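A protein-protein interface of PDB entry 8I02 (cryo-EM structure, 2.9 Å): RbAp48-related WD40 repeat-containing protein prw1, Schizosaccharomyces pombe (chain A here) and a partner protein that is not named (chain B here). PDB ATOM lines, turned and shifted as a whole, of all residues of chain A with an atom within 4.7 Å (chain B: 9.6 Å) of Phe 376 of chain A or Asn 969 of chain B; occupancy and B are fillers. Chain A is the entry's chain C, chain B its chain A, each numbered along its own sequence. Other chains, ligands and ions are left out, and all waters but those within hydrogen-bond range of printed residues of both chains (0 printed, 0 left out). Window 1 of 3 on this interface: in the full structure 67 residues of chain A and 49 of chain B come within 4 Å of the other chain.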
ATOM      1  N   LEU A  40     -32.907 -21.931   2.152  1.00  0.00           N
ATOM      2  CA  LEU A  40     -31.833 -21.124   2.712  1.00  0.00           C
ATOM      3  C   LEU A  40     -31.653 -19.783   2.009  1.00  0.00           C
ATOM      4  O   LEU A  40     -31.276 -18.806   2.657  1.00  0.00           O
ATOM      5  CB  LEU A  40     -30.516 -21.907   2.663  1.00  0.00           C
ATOM      6  CG  LEU A  40     -30.430 -23.272   3.343  1.00  0.00           C
ATOM      7  CD1 LEU A  40     -29.747 -24.285   2.448  1.00  0.00           C
ATOM      8  CD2 LEU A  40     -29.686 -23.143   4.649  1.00  0.00           C
ATOM      9  N   TYR A  41     -31.921 -19.696   0.712  1.00  0.00           N
ATOM     10  CA  TYR A  41     -31.624 -18.496  -0.054  1.00  0.00           C
ATOM     11  C   TYR A  41     -32.872 -17.957  -0.736  1.00  0.00           C
ATOM     12  O   TYR A  41     -33.655 -18.719  -1.304  1.00  0.00           O
ATOM     13  CB  TYR A  41     -30.567 -18.777  -1.113  1.00  0.00           C
ATOM     14  CG  TYR A  41     -29.308 -19.443  -0.621  1.00  0.00           C
ATOM     15  CD1 TYR A  41     -28.257 -18.698  -0.133  1.00  0.00           C
ATOM     16  CD2 TYR A  41     -29.155 -20.814  -0.687  1.00  0.00           C
ATOM     17  CE1 TYR A  41     -27.106 -19.293   0.293  1.00  0.00           C
ATOM     18  CE2 TYR A  41     -28.004 -21.415  -0.263  1.00  0.00           C
ATOM     19  CZ  TYR A  41     -26.985 -20.647   0.223  1.00  0.00           C
ATOM     20  OH  TYR A  41     -25.826 -21.238   0.651  1.00  0.00           O
ATOM     21  N   THR A 350     -18.665 -21.405   3.751  1.00  0.00           N
ATOM     22  CA  THR A 350     -18.634 -19.968   4.003  1.00  0.00           C
ATOM     23  C   THR A 350     -19.502 -19.692   5.222  1.00  0.00           C
ATOM     24  O   THR A 350     -20.724 -19.844   5.163  1.00  0.00           O
ATOM     25  CB  THR A 350     -19.140 -19.195   2.788  1.00  0.00           C
ATOM     26  OG1 THR A 350     -18.207 -19.334   1.711  1.00  0.00           O
ATOM     27  CG2 THR A 350     -19.331 -17.724   3.110  1.00  0.00           C
ATOM     28  N   LEU A 351     -18.875 -19.291   6.321  1.00  0.00           N
ATOM     29  CA  LEU A 351     -19.564 -19.109   7.590  1.00  0.00           C
ATOM     30  C   LEU A 351     -19.815 -17.626   7.816  1.00  0.00           C
ATOM     31  O   LEU A 351     -18.866 -16.843   7.912  1.00  0.00           O
ATOM     32  CB  LEU A 351     -18.753 -19.701   8.742  1.00  0.00           C
ATOM     33  CG  LEU A 351     -18.406 -21.193   8.723  1.00  0.00           C
ATOM     34  CD1 LEU A 351     -17.857 -21.593  10.048  1.00  0.00           C
ATOM     35  CD2 LEU A 351     -19.587 -22.047   8.401  1.00  0.00           C
ATOM     36  N   VAL A 352     -21.084 -17.245   7.885  1.00  0.00           N
ATOM     37  CA  VAL A 352     -21.498 -15.879   8.180  1.00  0.00           C
ATOM     38  C   VAL A 352     -21.872 -15.817   9.649  1.00  0.00           C
ATOM     39  O   VAL A 352     -22.753 -16.565  10.094  1.00  0.00           O
ATOM     40  CB  VAL A 352     -22.682 -15.452   7.299  1.00  0.00           C
ATOM     41  CG1 VAL A 352     -23.221 -14.113   7.740  1.00  0.00           C
ATOM     42  CG2 VAL A 352     -22.272 -15.413   5.848  1.00  0.00           C
ATOM     43  N   LEU A 374     -22.229 -18.509  15.086  1.00  0.00           N
ATOM     44  CA  LEU A 374     -22.501 -19.018  13.747  1.00  0.00           C
ATOM     45  C   LEU A 374     -23.939 -18.744  13.336  1.00  0.00           C
ATOM     46  O   LEU A 374     -24.878 -19.178  14.006  1.00  0.00           O
ATOM     47  CB  LEU A 374     -22.213 -20.517  13.716  1.00  0.00           C
ATOM     48  CG  LEU A 374     -22.206 -21.221  12.369  1.00  0.00           C
ATOM     49  CD1 LEU A 374     -21.021 -20.770  11.572  1.00  0.00           C
ATOM     50  CD2 LEU A 374     -22.163 -22.716  12.574  1.00  0.00           C
ATOM     51  N   LEU A 375     -24.109 -18.016  12.233  1.00  0.00           N
ATOM     52  CA  LEU A 375     -25.417 -17.561  11.784  1.00  0.00           C
ATOM     53  C   LEU A 375     -25.859 -18.157  10.455  1.00  0.00           C
ATOM     54  O   LEU A 375     -27.062 -18.276  10.217  1.00  0.00           O
ATOM     55  CB  LEU A 375     -25.430 -16.034  11.667  1.00  0.00           C
ATOM     56  CG  LEU A 375     -26.705 -15.384  11.144  1.00  0.00           C
ATOM     57  CD1 LEU A 375     -27.855 -15.642  12.087  1.00  0.00           C
ATOM     58  CD2 LEU A 375     -26.505 -13.903  10.941  1.00  0.00           C
ATOM     59  N   PHE A 376     -24.922 -18.525   9.585  1.00  0.00           N
ATOM     60  CA  PHE A 376     -25.286 -19.099   8.295  1.00  0.00           C
ATOM     61  C   PHE A 376     -24.081 -19.851   7.759  1.00  0.00           C
ATOM     62  O   PHE A 376     -22.942 -19.464   8.014  1.00  0.00           O
ATOM     63  CB  PHE A 376     -25.748 -18.000   7.315  1.00  0.00           C
ATOM     64  CG  PHE A 376     -26.451 -18.514   6.083  1.00  0.00           C
ATOM     65  CD1 PHE A 376     -25.730 -18.948   4.991  1.00  0.00           C
ATOM     66  CD2 PHE A 376     -27.828 -18.529   6.006  1.00  0.00           C
ATOM     67  CE1 PHE A 376     -26.362 -19.412   3.874  1.00  0.00           C
ATOM     68  CE2 PHE A 376     -28.460 -18.995   4.883  1.00  0.00           C
ATOM     69  CZ  PHE A 376     -27.729 -19.436   3.826  1.00  0.00           C
ATOM     70  N   MET A 377     -24.340 -20.930   7.023  1.00  0.00           N
ATOM     71  CA  MET A 377     -23.289 -21.684   6.347  1.00  0.00           C
ATOM     72  C   MET A 377     -23.645 -21.881   4.881  1.00  0.00           C
ATOM     73  O   MET A 377     -24.762 -22.294   4.556  1.00  0.00           O
ATOM     74  CB  MET A 377     -23.047 -23.049   6.995  1.00  0.00           C
ATOM     75  CG  MET A 377     -21.912 -23.813   6.333  1.00  0.00           C
ATOM     76  SD  MET A 377     -21.993 -25.598   6.453  1.00  0.00           S
ATOM     77  CE  MET A 377     -21.702 -25.823   8.189  1.00  0.00           C
ATOM     78  N   HIS A 378     -22.685 -21.600   4.002  1.00  0.00           N
ATOM     79  CA  HIS A 378     -22.828 -21.777   2.562  1.00  0.00           C
ATOM     80  C   HIS A 378     -21.928 -22.921   2.122  1.00  0.00           C
ATOM     81  O   HIS A 378     -20.709 -22.855   2.300  1.00  0.00           O
ATOM     82  CB  HIS A 378     -22.469 -20.491   1.814  1.00  0.00           C
ATOM     83  CG  HIS A 378     -22.451 -20.634   0.323  1.00  0.00           C
ATOM     84  ND1 HIS A 378     -23.496 -21.180  -0.387  1.00  0.00           N
ATOM     85  CD2 HIS A 378     -21.519 -20.284  -0.592  1.00  0.00           C
ATOM     86  CE1 HIS A 378     -23.205 -21.171  -1.674  1.00  0.00           C
ATOM     87  NE2 HIS A 378     -22.012 -20.630  -1.825  1.00  0.00           N
ATOM     88  N   TRP A 410     -25.268 -14.950  -3.950  1.00  0.00           N
ATOM     89  CA  TRP A 410     -26.309 -15.502  -3.099  1.00  0.00           C
ATOM     90  C   TRP A 410     -26.723 -14.524  -2.011  1.00  0.00           C
ATOM     91  O   TRP A 410     -25.945 -13.667  -1.581  1.00  0.00           O
ATOM     92  CB  TRP A 410     -25.883 -16.836  -2.466  1.00  0.00           C
ATOM     93  CG  TRP A 410     -24.528 -16.863  -1.851  1.00  0.00           C
ATOM     94  CD1 TRP A 410     -23.370 -17.221  -2.456  1.00  0.00           C
ATOM     95  CD2 TRP A 410     -24.194 -16.556  -0.496  1.00  0.00           C
ATOM     96  NE1 TRP A 410     -22.331 -17.135  -1.572  1.00  0.00           N
ATOM     97  CE2 TRP A 410     -22.817 -16.731  -0.359  1.00  0.00           C
ATOM     98  CE3 TRP A 410     -24.929 -16.143   0.612  1.00  0.00           C
ATOM     99  CZ2 TRP A 410     -22.162 -16.507   0.833  1.00  0.00           C
ATOM    100  CZ3 TRP A 410     -24.275 -15.920   1.790  1.00  0.00           C
ATOM    101  CH2 TRP A 410     -22.913 -16.107   1.894  1.00  0.00           C
ATOM    102  N   PRO A 412     -28.857 -14.911   1.732  1.00  0.00           N
ATOM    103  CA  PRO A 412     -29.583 -15.737   2.699  1.00  0.00           C
ATOM    104  C   PRO A 412     -31.034 -15.302   2.836  1.00  0.00           C
ATOM    105  O   PRO A 412     -31.400 -14.161   2.555  1.00  0.00           O
ATOM    106  CB  PRO A 412     -28.817 -15.505   4.001  1.00  0.00           C
ATOM    107  CG  PRO A 412     -27.469 -15.072   3.574  1.00  0.00           C
ATOM    108  CD  PRO A 412     -27.648 -14.308   2.319  1.00  0.00           C
ATOM    109  N   SER A 413     -31.867 -16.230   3.296  1.00  0.00           N
ATOM    110  CA  SER A 413     -33.283 -15.940   3.455  1.00  0.00           C
ATOM    111  C   SER A 413     -33.498 -14.819   4.457  1.00  0.00           C
ATOM    112  O   SER A 413     -32.612 -14.450   5.222  1.00  0.00           O
ATOM    113  CB  SER A 413     -34.050 -17.170   3.920  1.00  0.00           C
ATOM    114  OG  SER A 413     -33.844 -18.262   3.056  1.00  0.00           O
ATOM    115  N   SER A 415     -35.843 -15.170   6.780  1.00  0.00           N
ATOM    116  CA  SER A 415     -36.118 -15.945   7.981  1.00  0.00           C
ATOM    117  C   SER A 415     -34.874 -16.267   8.790  1.00  0.00           C
ATOM    118  O   SER A 415     -34.988 -16.918   9.831  1.00  0.00           O
ATOM    119  CB  SER A 415     -36.808 -17.248   7.596  1.00  0.00           C
ATOM    120  OG  SER A 415     -35.868 -18.303   7.522  1.00  0.00           O
ATOM    121  N   ILE A 416     -33.698 -15.850   8.335  1.00  0.00           N
ATOM    122  CA  ILE A 416     -32.446 -16.158   8.997  1.00  0.00           C
ATOM    123  C   ILE A 416     -31.801 -14.915   9.589  1.00  0.00           C
ATOM    124  O   ILE A 416     -31.315 -14.949  10.720  1.00  0.00           O
ATOM    125  CB  ILE A 416     -31.494 -16.871   8.024  1.00  0.00           C
ATOM    126  CG1 ILE A 416     -32.012 -18.273   7.755  1.00  0.00           C
ATOM    127  CG2 ILE A 416     -30.101 -16.907   8.575  1.00  0.00           C
ATOM    128  CD1 ILE A 416     -31.321 -18.952   6.656  1.00  0.00           C
ATOM    129  N   ARG B 892     -34.164 -34.714  11.528  1.00  0.00           N
ATOM    130  CA  ARG B 892     -32.867 -34.176  11.144  1.00  0.00           C
ATOM    131  C   ARG B 892     -31.752 -35.125  11.517  1.00  0.00           C
ATOM    132  O   ARG B 892     -30.871 -35.401  10.699  1.00  0.00           O
ATOM    133  CB  ARG B 892     -32.633 -32.832  11.810  1.00  0.00           C
ATOM    134  CG  ARG B 892     -33.276 -31.678  11.106  1.00  0.00           C
ATOM    135  CD  ARG B 892     -33.570 -30.605  12.108  1.00  0.00           C
ATOM    136  NE  ARG B 892     -33.945 -29.345  11.496  1.00  0.00           N
ATOM    137  CZ  ARG B 892     -34.430 -28.326  12.185  1.00  0.00           C
ATOM    138  NH1 ARG B 892     -34.598 -28.434  13.495  1.00  0.00           N
ATOM    139  NH2 ARG B 892     -34.745 -27.207  11.566  1.00  0.00           N
ATOM    140  N   GLU B 896     -31.011 -36.203   7.829  1.00  0.00           N
ATOM    141  CA  GLU B 896     -30.119 -35.181   7.286  1.00  0.00           C
ATOM    142  C   GLU B 896     -28.832 -35.016   8.081  1.00  0.00           C
ATOM    143  O   GLU B 896     -28.138 -34.018   7.895  1.00  0.00           O
ATOM    144  CB  GLU B 896     -30.829 -33.826   7.208  1.00  0.00           C
ATOM    145  CG  GLU B 896     -31.345 -33.467   5.834  1.00  0.00           C
ATOM    146  CD  GLU B 896     -32.658 -32.723   5.897  1.00  0.00           C
ATOM    147  OE1 GLU B 896     -33.558 -33.001   5.078  1.00  0.00           O
ATOM    148  OE2 GLU B 896     -32.790 -31.862   6.785  1.00  0.00           O
ATOM    149  N   CYS B 963     -22.329 -32.117   6.213  1.00  0.00           N
ATOM    150  CA  CYS B 963     -23.621 -31.567   5.812  1.00  0.00           C
ATOM    151  C   CYS B 963     -23.350 -30.440   4.826  1.00  0.00           C
ATOM    152  O   CYS B 963     -22.294 -29.800   4.904  1.00  0.00           O
ATOM    153  CB  CYS B 963     -24.434 -31.048   7.003  1.00  0.00           C
ATOM    154  SG  CYS B 963     -26.238 -31.004   6.781  1.00  0.00           S
ATOM    155  N   PRO B 964     -24.257 -30.149   3.903  1.00  0.00           N
ATOM    156  CA  PRO B 964     -24.158 -28.892   3.158  1.00  0.00           C
ATOM    157  C   PRO B 964     -24.487 -27.675   4.002  1.00  0.00           C
ATOM    158  O   PRO B 964     -23.731 -26.706   4.016  1.00  0.00           O
ATOM    159  CB  PRO B 964     -25.179 -29.075   2.033  1.00  0.00           C
ATOM    160  CG  PRO B 964     -25.338 -30.518   1.902  1.00  0.00           C
ATOM    161  CD  PRO B 964     -25.220 -31.064   3.281  1.00  0.00           C
ATOM    162  N   PHE B 965     -25.604 -27.710   4.715  1.00  0.00           N
ATOM    163  CA  PHE B 965     -26.190 -26.519   5.309  1.00  0.00           C
ATOM    164  C   PHE B 965     -26.320 -26.669   6.820  1.00  0.00           C
ATOM    165  O   PHE B 965     -25.794 -27.601   7.423  1.00  0.00           O
ATOM    166  CB  PHE B 965     -27.540 -26.215   4.661  1.00  0.00           C
ATOM    167  CG  PHE B 965     -28.511 -27.363   4.682  1.00  0.00           C
ATOM    168  CD1 PHE B 965     -28.439 -28.366   3.742  1.00  0.00           C
ATOM    169  CD2 PHE B 965     -29.524 -27.410   5.615  1.00  0.00           C
ATOM    170  CE1 PHE B 965     -29.323 -29.400   3.754  1.00  0.00           C
ATOM    171  CE2 PHE B 965     -30.412 -28.442   5.624  1.00  0.00           C
ATOM    172  CZ  PHE B 965     -30.310 -29.438   4.691  1.00  0.00           C
ATOM    173  N   LEU B 966     -27.009 -25.714   7.427  1.00  0.00           N
ATOM    174  CA  LEU B 966     -27.201 -25.634   8.871  1.00  0.00           C
ATOM    175  C   LEU B 966     -28.667 -25.923   9.168  1.00  0.00           C
ATOM    176  O   LEU B 966     -29.542 -25.142   8.788  1.00  0.00           O
ATOM    177  CB  LEU B 966     -26.807 -24.248   9.370  1.00  0.00           C
ATOM    178  CG  LEU B 966     -26.268 -24.060  10.771  1.00  0.00           C
ATOM    179  CD1 LEU B 966     -24.831 -24.444  10.770  1.00  0.00           C
ATOM    180  CD2 LEU B 966     -26.417 -22.632  11.208  1.00  0.00           C
ATOM    181  N   CYS B 967     -28.940 -27.025   9.861  1.00  0.00           N
ATOM    182  CA  CYS B 967     -30.321 -27.465  10.022  1.00  0.00           C
ATOM    183  C   CYS B 967     -31.171 -26.482  10.816  1.00  0.00           C
ATOM    184  O   CYS B 967     -32.400 -26.552  10.745  1.00  0.00           O
ATOM    185  CB  CYS B 967     -30.361 -28.840  10.682  1.00  0.00           C
ATOM    186  SG  CYS B 967     -29.472 -30.131   9.787  1.00  0.00           S
ATOM    187  N   ARG B 968     -30.553 -25.577  11.580  1.00  0.00           N
ATOM    188  CA  ARG B 968     -31.332 -24.536  12.242  1.00  0.00           C
ATOM    189  C   ARG B 968     -32.007 -23.628  11.231  1.00  0.00           C
ATOM    190  O   ARG B 968     -33.051 -23.039  11.523  1.00  0.00           O
ATOM    191  CB  ARG B 968     -30.463 -23.655  13.139  1.00  0.00           C
ATOM    192  CG  ARG B 968     -29.384 -24.294  13.949  1.00  0.00           C
ATOM    193  CD  ARG B 968     -28.552 -23.174  14.537  1.00  0.00           C
ATOM    194  NE  ARG B 968     -27.433 -23.635  15.346  1.00  0.00           N
ATOM    195  CZ  ARG B 968     -26.414 -22.861  15.704  1.00  0.00           C
ATOM    196  NH1 ARG B 968     -26.379 -21.597  15.308  1.00  0.00           N
ATOM    197  NH2 ARG B 968     -25.433 -23.349  16.448  1.00  0.00           N
ATOM    198  N   ASN B 969     -31.409 -23.480  10.053  1.00  0.00           N
ATOM    199  CA  ASN B 969     -31.818 -22.434   9.132  1.00  0.00           C
ATOM    200  C   ASN B 969     -33.153 -22.726   8.465  1.00  0.00           C
ATOM    201  O   ASN B 969     -33.891 -21.791   8.147  1.00  0.00           O
ATOM    202  CB  ASN B 969     -30.749 -22.238   8.060  1.00  0.00           C
ATOM    203  CG  ASN B 969     -29.471 -21.653   8.602  1.00  0.00           C
ATOM    204  OD1 ASN B 969     -29.439 -21.084   9.691  1.00  0.00           O
ATOM    205  ND2 ASN B 969     -28.406 -21.771   7.828  1.00  0.00           N
ATOM    206  N   ILE B 970     -33.481 -23.995   8.246  1.00  0.00           N
ATOM    207  CA  ILE B 970     -34.642 -24.362   7.452  1.00  0.00           C
ATOM    208  C   ILE B 970     -35.810 -24.801   8.333  1.00  0.00           C
ATOM    209  O   ILE B 970     -36.710 -25.489   7.866  1.00  0.00           O
ATOM    210  CB  ILE B 970     -34.291 -25.435   6.411  1.00  0.00           C
ATOM    211  CG1 ILE B 970     -34.126 -26.795   7.053  1.00  0.00           C
ATOM    212  CG2 ILE B 970     -32.987 -25.116   5.750  1.00  0.00           C
ATOM    213  CD1 ILE B 970     -33.846 -27.868   6.051  1.00  0.00           C
ATOM    214  N   GLU B 971     -35.822 -24.387   9.591  1.00  0.00           N
ATOM    215  CA  GLU B 971     -36.784 -24.892  10.567  1.00  0.00           C
ATOM    216  C   GLU B 971     -38.172 -24.359  10.258  1.00  0.00           C
ATOM    217  O   GLU B 971     -38.441 -23.169  10.425  1.00  0.00           O
ATOM    218  CB  GLU B 971     -36.367 -24.505  11.983  1.00  0.00           C
ATOM    219  CG  GLU B 971     -37.483 -24.626  13.013  1.00  0.00           C
ATOM    220  CD  GLU B 971     -37.776 -26.062  13.405  1.00  0.00           C
ATOM    221  OE1 GLU B 971     -37.581 -26.410  14.588  1.00  0.00           O
ATOM    222  OE2 GLU B 971     -38.200 -26.841  12.530  1.00  0.00           O
ATOM    223  N   LYS B 972     -39.050 -25.223   9.749  1.00  0.00           N
ATOM    224  CA  LYS B 972     -40.472 -24.915   9.807  1.00  0.00           C
ATOM    225  C   LYS B 972     -41.333 -26.019  10.425  1.00  0.00           C
ATOM    226  O   LYS B 972     -42.056 -25.776  11.395  1.00  0.00           O
ATOM    227  CB  LYS B 972     -40.981 -24.588   8.403  1.00  0.00           C
ATOM    228  CG  LYS B 972     -40.400 -23.317   7.810  1.00  0.00           C
ATOM    229  CD  LYS B 972     -41.010 -22.996   6.454  1.00  0.00           C
ATOM    230  CE  LYS B 972     -40.338 -23.768   5.330  1.00  0.00           C
ATOM    231  NZ  LYS B 972     -40.632 -25.228   5.359  1.00  0.00           N
ATOM    232  N   GLU B 973     -41.212 -27.243   9.911  1.00  0.00           N
ATOM    233  CA  GLU B 973     -42.354 -28.140   9.778  1.00  0.00           C
ATOM    234  C   GLU B 973     -42.395 -29.239  10.832  1.00  0.00           C
ATOM    235  O   GLU B 973     -41.480 -29.418  11.632  1.00  0.00           O
ATOM    236  CB  GLU B 973     -42.368 -28.763   8.380  1.00  0.00           C
ATOM    237  CG  GLU B 973     -42.692 -27.782   7.269  1.00  0.00           C
ATOM    238  CD  GLU B 973     -43.972 -27.006   7.518  1.00  0.00           C
ATOM    239  OE1 GLU B 973     -43.890 -25.853   7.989  1.00  0.00           O
ATOM    240  OE2 GLU B 973     -45.061 -27.545   7.233  1.00  0.00           O
ATOM    241  N   LEU B 979     -42.910 -31.232   5.090  1.00  0.00           N
ATOM    242  CA  LEU B 979     -41.717 -30.543   4.615  1.00  0.00           C
ATOM    243  C   LEU B 979     -41.617 -30.608   3.097  1.00  0.00           C
ATOM    244  O   LEU B 979     -41.341 -29.598   2.437  1.00  0.00           O
ATOM    245  CB  LEU B 979     -40.480 -31.155   5.268  1.00  0.00           C
ATOM    246  CG  LEU B 979     -39.173 -30.378   5.262  1.00  0.00           C
ATOM    247  CD1 LEU B 979     -39.248 -29.240   6.236  1.00  0.00           C
ATOM    248  CD2 LEU B 979     -38.031 -31.297   5.607  1.00  0.00           C
ATOM    249  N   LYS B 986     -43.241 -23.949  -2.457  1.00  0.00           N
ATOM    250  CA  LYS B 986     -42.261 -22.879  -2.584  1.00  0.00           C
ATOM    251  C   LYS B 986     -41.680 -22.808  -3.979  1.00  0.00           C
ATOM    252  O   LYS B 986     -41.248 -21.737  -4.402  1.00  0.00           O
ATOM    253  CB  LYS B 986     -41.125 -23.073  -1.582  1.00  0.00           C
ATOM    254  CG  LYS B 986     -40.997 -21.949  -0.595  1.00  0.00           C
ATOM    255  CD  LYS B 986     -39.917 -22.227   0.413  1.00  0.00           C
ATOM    256  CE  LYS B 986     -39.702 -21.020   1.288  1.00  0.00           C
ATOM    257  NZ  LYS B 986     -40.962 -20.620   1.957  1.00  0.00           N
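The backbone NH (N) of Leu 375 of chain A lies within hydrogen-bond range of the backbone carbonyl oxygen (O) of Val 352 of chain A. The backbone carbonyl oxygen of Phe 965 of chain B is in hydrogen-bond range of the side-chain sulfur of Cys 963 of chain B, at 3.5 Å. The backbone NH (N) of Val 352 of chain A lies within hydrogen-bond range of the backbone carbonyl oxygen (O) of Phe 376 of chain A (2.9 Å). OG of Ser 413 of chain A lies within hydrogen-bond range of O of Leu 40 of chain A (2.7 Å).
Phe 965 of chain B touches Leu 40 of chain A. Leu 40 of chain A touches Asn 969 of chain B. Leu 40 of chain A touches Ile 970 of chain B (CG to CG2, 3.97 Å). CD1 of Leu 966 of chain B touches CD2 of Leu 374 of chain A, at 3.7 Å. Leu 375 of chain A touches Asn 969 of chain B (O to OD1, 3.7 Å). Phe 376 of chain A touches Asn 969 of chain B. CD1 of Ile 416 of chain A touches CB of Asn 969 of chain B, 3.6 Å away.
Printed residues of chain B that touch a printed residue of chain A: Pro 964, Phe 965, Leu 966, Arg 968, Asn 969 and Ile 970. Hydrophobic or aromatic side chains of chain B that line the printed part of chain A: Phe 965, Leu 966 and Ile 970. Of the 15 printed residues of chain A, 6 touch a printed residue of chain B. Printed residues of chain A that touch a printed residue of chain B: Leu 40, Leu 374, Leu 375, Phe 376, Met 377 and Ile 416. Hydrophobic or aromatic side chains of chain A that line the printed part of chain B: Leu 40, Leu 374, Phe 376, Met 377 and Ile 416. Among the printed residues, 9 pairs touch across the chains.
Of the printed residues of chain B, Leu 40 of chain A touches Phe 965 (3.7 Å), Asn 969 (3.7 Å) and Ile 970 (3.97 Å). Of chain B, only Asn 969 comes within 4 Å of Leu 375 of chain A. Phe 376 of chain A touches just one residue of chain B: Asn 969 (3.8 Å). Printed residues of chain B within 4 Å of Ile 416 of chain A: Asn 969. Of the printed residues of chain A, Phe 965 of chain B touches Leu 40. Asn 969 of chain B touches four residues of chain A. Glu 973 of chain B touches none of the printed residues of chain A. Lys 986 of chain B touches none of the printed residues of chain A. The nearest printed residue of chain A that does not touch Leu 966 of chain B is Met 377 of chain A (4.3 Å).
O of Leu 374 of chain A is in hydrogen-bond range of NH1 of Arg 968 of chain B, at 3.1 Å. The backbone carbonyl oxygen (O) of Pro 964 of chain B lies close to the side-chain sulfur (SD) of Met 377 of chain A.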
